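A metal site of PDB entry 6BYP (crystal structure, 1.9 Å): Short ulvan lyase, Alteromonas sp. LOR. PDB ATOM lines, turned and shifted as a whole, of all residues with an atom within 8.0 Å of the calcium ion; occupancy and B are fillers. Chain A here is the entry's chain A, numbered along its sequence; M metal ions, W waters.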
ATOM      1  N   ASN A 250       1.118   6.540 -24.104  1.00  0.00           N
ATOM      2  CA  ASN A 250       1.635   5.500 -23.209  1.00  0.00           C
ATOM      3  C   ASN A 250       0.811   4.219 -23.255  1.00  0.00           C
ATOM      4  O   ASN A 250       0.838   3.435 -22.296  1.00  0.00           O
ATOM      5  CB  ASN A 250       1.676   5.991 -21.763  1.00  0.00           C
ATOM      6  CG  ASN A 250       0.347   6.501 -21.296  1.00  0.00           C
ATOM      7  OD1 ASN A 250      -0.699   6.027 -21.736  1.00  0.00           O
ATOM      8  ND2 ASN A 250       0.368   7.428 -20.346  1.00  0.00           N
ATOM      9  N   GLN A 305      10.284   2.693 -25.272  1.00  0.00           N
ATOM     10  CA  GLN A 305       8.936   2.622 -24.742  1.00  0.00           C
ATOM     11  C   GLN A 305       8.576   3.941 -24.064  1.00  0.00           C
ATOM     12  O   GLN A 305       9.446   4.704 -23.624  1.00  0.00           O
ATOM     13  CB  GLN A 305       8.804   1.487 -23.727  1.00  0.00           C
ATOM     14  CG  GLN A 305       9.388   1.816 -22.346  1.00  0.00           C
ATOM     15  CD  GLN A 305       8.985   0.777 -21.296  1.00  0.00           C
ATOM     16  OE1 GLN A 305       8.350  -0.219 -21.642  1.00  0.00           O
ATOM     17  NE2 GLN A 305       9.332   1.006 -20.025  1.00  0.00           N
ATOM     18  N   ARG A 306       7.279   4.195 -23.975  1.00  0.00           N
ATOM     19  CA  ARG A 306       6.765   5.239 -23.099  1.00  0.00           C
ATOM     20  C   ARG A 306       5.840   4.558 -22.101  1.00  0.00           C
ATOM     21  O   ARG A 306       4.694   4.251 -22.419  1.00  0.00           O
ATOM     22  CB  ARG A 306       6.019   6.341 -23.874  1.00  0.00           C
ATOM     23  CG  ARG A 306       5.436   7.413 -22.945  1.00  0.00           C
ATOM     24  CD  ARG A 306       4.730   8.556 -23.715  1.00  0.00           C
ATOM     25  NE  ARG A 306       5.646   9.233 -24.641  1.00  0.00           N
ATOM     26  CZ  ARG A 306       5.321  10.276 -25.404  1.00  0.00           C
ATOM     27  NH1 ARG A 306       4.095  10.795 -25.359  1.00  0.00           N
ATOM     28  NH2 ARG A 306       6.235  10.810 -26.211  1.00  0.00           N
ATOM     29  N   SER A 307       6.353   4.345 -20.885  1.00  0.00           N
ATOM     30  CA  SER A 307       5.525   3.752 -19.850  1.00  0.00           C
ATOM     31  C   SER A 307       4.459   4.737 -19.372  1.00  0.00           C
ATOM     32  O   SER A 307       4.669   5.950 -19.348  1.00  0.00           O
ATOM     33  CB  SER A 307       6.380   3.311 -18.661  1.00  0.00           C
ATOM     34  OG  SER A 307       5.537   2.943 -17.577  1.00  0.00           O
ATOM     35  N   ALA A 308       3.317   4.186 -18.963  1.00  0.00           N
ATOM     36  CA  ALA A 308       2.280   5.007 -18.359  1.00  0.00           C
ATOM     37  C   ALA A 308       2.621   5.410 -16.934  1.00  0.00           C
ATOM     38  O   ALA A 308       1.903   6.224 -16.344  1.00  0.00           O
ATOM     39  CB  ALA A 308       0.935   4.267 -18.402  1.00  0.00           C
ATOM     40  N   ASN A 309       3.692   4.875 -16.359  1.00  0.00           N
ATOM     41  CA  ASN A 309       4.168   5.285 -15.057  1.00  0.00           C
ATOM     42  C   ASN A 309       4.596   6.744 -15.112  1.00  0.00           C
ATOM     43  O   ASN A 309       5.470   7.109 -15.896  1.00  0.00           O
ATOM     44  CB  ASN A 309       5.338   4.404 -14.630  1.00  0.00           C
ATOM     45  CG  ASN A 309       5.784   4.662 -13.224  1.00  0.00           C
ATOM     46  OD1 ASN A 309       5.360   5.629 -12.583  1.00  0.00           O
ATOM     47  ND2 ASN A 309       6.661   3.797 -12.717  1.00  0.00           N
ATOM     48  N   ASN A 310       3.988   7.591 -14.293  1.00  0.00           N
ATOM     49  CA  ASN A 310       4.343   8.998 -14.302  1.00  0.00           C
ATOM     50  C   ASN A 310       5.108   9.386 -13.044  1.00  0.00           C
ATOM     51  O   ASN A 310       5.297  10.583 -12.770  1.00  0.00           O
ATOM     52  CB  ASN A 310       3.094   9.866 -14.502  1.00  0.00           C
ATOM     53  CG  ASN A 310       2.513   9.740 -15.934  1.00  0.00           C
ATOM     54  OD1 ASN A 310       3.259   9.547 -16.910  1.00  0.00           O
ATOM     55  ND2 ASN A 310       1.190   9.858 -16.048  1.00  0.00           N
ATOM     56  N   ASP A 311       5.606   8.394 -12.305  1.00  0.00           N
ATOM     57  CA  ASP A 311       6.341   8.624 -11.081  1.00  0.00           C
ATOM     58  C   ASP A 311       7.819   8.265 -11.179  1.00  0.00           C
ATOM     59  O   ASP A 311       8.558   8.513 -10.219  1.00  0.00           O
ATOM     60  CB  ASP A 311       5.720   7.824  -9.931  1.00  0.00           C
ATOM     61  CG  ASP A 311       4.302   8.282  -9.582  1.00  0.00           C
ATOM     62  OD1 ASP A 311       3.986   9.483  -9.706  1.00  0.00           O
ATOM     63  OD2 ASP A 311       3.501   7.423  -9.151  1.00  0.00           O
ATOM     64  N   ASP A 312       8.278   7.677 -12.279  1.00  0.00           N
ATOM     65  CA  ASP A 312       9.702   7.372 -12.400  1.00  0.00           C
ATOM     66  C   ASP A 312      10.420   8.543 -13.058  1.00  0.00           C
ATOM     67  O   ASP A 312       9.839   9.592 -13.342  1.00  0.00           O
ATOM     68  CB  ASP A 312       9.924   6.051 -13.148  1.00  0.00           C
ATOM     69  CG  ASP A 312       9.523   6.122 -14.621  1.00  0.00           C
ATOM     70  OD1 ASP A 312       9.072   7.180 -15.099  1.00  0.00           O
ATOM     71  OD2 ASP A 312       9.644   5.078 -15.291  1.00  0.00           O
ATOM     72  N   ARG A 313      11.726   8.375 -13.282  1.00  0.00           N
ATOM     73  CA  ARG A 313      12.536   9.501 -13.731  1.00  0.00           C
ATOM     74  C   ARG A 313      12.285   9.880 -15.195  1.00  0.00           C
ATOM     75  O   ARG A 313      12.751  10.948 -15.610  1.00  0.00           O
ATOM     76  CB  ARG A 313      14.030   9.178 -13.521  1.00  0.00           C
ATOM     77  CG  ARG A 313      14.618   8.193 -14.536  1.00  0.00           C
ATOM     78  CD  ARG A 313      16.042   7.765 -14.152  1.00  0.00           C
ATOM     79  NE  ARG A 313      16.022   6.864 -13.003  1.00  0.00           N
ATOM     80  CZ  ARG A 313      17.106   6.393 -12.389  1.00  0.00           C
ATOM     81  NH1 ARG A 313      18.321   6.747 -12.816  1.00  0.00           N
ATOM     82  NH2 ARG A 313      16.990   5.589 -11.344  1.00  0.00           N
ATOM     83  N   PHE A 314      11.595   9.062 -15.972  1.00  0.00           N
ATOM     84  CA  PHE A 314      11.480   9.290 -17.414  1.00  0.00           C
ATOM     85  C   PHE A 314      10.195  10.052 -17.711  1.00  0.00           C
ATOM     86  O   PHE A 314       9.095   9.524 -17.531  1.00  0.00           O
ATOM     87  CB  PHE A 314      11.511   7.952 -18.160  1.00  0.00           C
ATOM     88  CG  PHE A 314      12.773   7.185 -17.899  1.00  0.00           C
ATOM     89  CD1 PHE A 314      13.954   7.578 -18.497  1.00  0.00           C
ATOM     90  CD2 PHE A 314      12.780   6.103 -17.035  1.00  0.00           C
ATOM     91  CE1 PHE A 314      15.148   6.884 -18.254  1.00  0.00           C
ATOM     92  CE2 PHE A 314      13.967   5.416 -16.784  1.00  0.00           C
ATOM     93  CZ  PHE A 314      15.141   5.801 -17.390  1.00  0.00           C
ATOM     94  N   LYS A 315      10.320  11.313 -18.133  1.00  0.00           N
ATOM     95  CA  LYS A 315       9.105  12.069 -18.436  1.00  0.00           C
ATOM     96  C   LYS A 315       8.369  11.455 -19.620  1.00  0.00           C
ATOM     97  O   LYS A 315       7.131  11.394 -19.629  1.00  0.00           O
ATOM     98  CB  LYS A 315       9.406  13.532 -18.711  1.00  0.00           C
ATOM     99  CG  LYS A 315       8.105  14.317 -18.909  1.00  0.00           C
ATOM    100  CD  LYS A 315       8.353  15.793 -18.985  1.00  0.00           C
ATOM    101  CE  LYS A 315       7.061  16.589 -19.131  1.00  0.00           C
ATOM    102  NZ  LYS A 315       7.391  18.052 -19.286  1.00  0.00           N
ATOM    103  N   TYR A 316       9.116  11.007 -20.650  1.00  0.00           N
ATOM    104  CA  TYR A 316       8.485  10.436 -21.827  1.00  0.00           C
ATOM    105  C   TYR A 316       9.038   9.041 -22.049  1.00  0.00           C
ATOM    106  O   TYR A 316       8.713   8.126 -21.270  1.00  0.00           O
ATOM    107  CB  TYR A 316       8.670  11.375 -23.038  1.00  0.00           C
ATOM    108  CG  TYR A 316       7.913  12.681 -22.869  1.00  0.00           C
ATOM    109  CD1 TYR A 316       6.520  12.691 -22.797  1.00  0.00           C
ATOM    110  CD2 TYR A 316       8.585  13.900 -22.795  1.00  0.00           C
ATOM    111  CE1 TYR A 316       5.816  13.887 -22.629  1.00  0.00           C
ATOM    112  CE2 TYR A 316       7.888  15.108 -22.633  1.00  0.00           C
ATOM    113  CZ  TYR A 316       6.511  15.087 -22.553  1.00  0.00           C
ATOM    114  OH  TYR A 316       5.837  16.275 -22.389  1.00  0.00           O
ATOM    115  N   GLN A 317       9.905   8.815 -23.047  1.00  0.00           N
ATOM    116  CA  GLN A 317      10.359   7.472 -23.346  1.00  0.00           C
ATOM    117  C   GLN A 317      11.496   7.064 -22.400  1.00  0.00           C
ATOM    118  O   GLN A 317      12.075   7.879 -21.681  1.00  0.00           O
ATOM    119  CB  GLN A 317      10.841   7.344 -24.791  1.00  0.00           C
ATOM    120  CG  GLN A 317       9.718   7.160 -25.836  1.00  0.00           C
ATOM    121  CD  GLN A 317       9.032   8.463 -26.256  1.00  0.00           C
ATOM    122  OE1 GLN A 317       8.193   8.985 -25.538  1.00  0.00           O
ATOM    123  NE2 GLN A 317       9.388   8.954 -27.436  1.00  0.00           N
ATOM    124  N   ASN A 318      11.793   5.776 -22.421  1.00  0.00           N
ATOM    125  CA  ASN A 318      12.975   5.215 -21.794  1.00  0.00           C
ATOM    126  C   ASN A 318      13.329   3.950 -22.548  1.00  0.00           C
ATOM    127  O   ASN A 318      12.509   3.406 -23.289  1.00  0.00           O
ATOM    128  CB  ASN A 318      12.763   4.934 -20.289  1.00  0.00           C
ATOM    129  CG  ASN A 318      12.021   3.642 -20.033  1.00  0.00           C
ATOM    130  OD1 ASN A 318      10.798   3.603 -19.995  1.00  0.00           O
ATOM    131  ND2 ASN A 318      12.767   2.569 -19.864  1.00  0.00           N
ATOM    132  N   PRO A 366      11.761  12.264 -10.168  1.00  0.00           N
ATOM    133  CA  PRO A 366      10.650  11.976 -11.089  1.00  0.00           C
ATOM    134  C   PRO A 366      10.630  12.917 -12.294  1.00  0.00           C
ATOM    135  O   PRO A 366      10.753  14.127 -12.157  1.00  0.00           O
ATOM    136  CB  PRO A 366       9.410  12.150 -10.206  1.00  0.00           C
ATOM    137  CG  PRO A 366       9.918  11.793  -8.820  1.00  0.00           C
ATOM    138  CD  PRO A 366      11.308  12.320  -8.767  1.00  0.00           C
ATOM    139  N   ASN A 367      10.522  12.328 -13.494  1.00  0.00           N
ATOM    140  CA  ASN A 367      10.346  13.048 -14.750  1.00  0.00           C
ATOM    141  C   ASN A 367      11.540  13.937 -15.108  1.00  0.00           C
ATOM    142  O   ASN A 367      11.430  14.820 -15.958  1.00  0.00           O
ATOM    143  CB  ASN A 367       9.065  13.878 -14.689  1.00  0.00           C
ATOM    144  CG  ASN A 367       7.868  12.998 -14.494  1.00  0.00           C
ATOM    145  OD1 ASN A 367       7.510  12.223 -15.387  1.00  0.00           O
ATOM    146  ND2 ASN A 367       7.274  13.068 -13.312  1.00  0.00           N
ATOM    147  N   VAL A 369      14.317  13.104 -16.658  1.00  0.00           N
ATOM    148  CA  VAL A 369      15.058  12.619 -17.824  1.00  0.00           C
ATOM    149  C   VAL A 369      14.123  12.623 -19.028  1.00  0.00           C
ATOM    150  O   VAL A 369      13.075  11.975 -19.018  1.00  0.00           O
ATOM    151  CB  VAL A 369      15.617  11.204 -17.596  1.00  0.00           C
ATOM    152  CG1 VAL A 369      16.310  10.712 -18.846  1.00  0.00           C
ATOM    153  CG2 VAL A 369      16.539  11.197 -16.377  1.00  0.00           C
HETATM  154 CA    CA M   1       7.444   8.082 -16.788  1.00  0.00          CA
HETATM  155  O   HOH W   1       5.946  10.032 -17.282  1.00  0.00           O
HETATM  156  O   HOH W   2       7.600   9.478 -14.870  1.00  0.00           O
HETATM  157  O   HOH W   3       6.772   7.865 -19.136  1.00  0.00           O
HETATM  158  O   HOH W   4       8.384   5.947 -17.514  1.00  0.00           O
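Within 4 Å of the calcium ion: Asn 309, Asp 312 and Phe 314.
Water W3 bridges the backbone carbonyl oxygen of Ser 307 (2.9 Å) and the backbone carbonyl oxygen of Tyr 316 (2.9 Å).
O of Phe 314 is bound to the calcium ion (2.3 Å). O of Asn 309 binds the calcium ion (2.4 Å). Water W2 is bound to the calcium ion. Water W4 is bound to the calcium ion (2.4 Å). Water W3 is bound to the calcium ion (2.5 Å). Water W1 binds the calcium ion, at 2.5 Å. The side-chain carboxylate (OD1) of Asp 312 is bound to the calcium ion, at 2.5 Å.
The backbone NH (N) of Asn 309 is in hydrogen-bond range of the side-chain hydroxyl (OG) of Ser 307 (2.9 Å). N of Asp 311 sits at hydrogen-bond distance from OD1 of Asn 309, 2.8 Å away. The backbone carbonyl oxygen of Asp 312 sits at hydrogen-bond distance from the backbone NH of Asn 367, 2.8 Å away.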
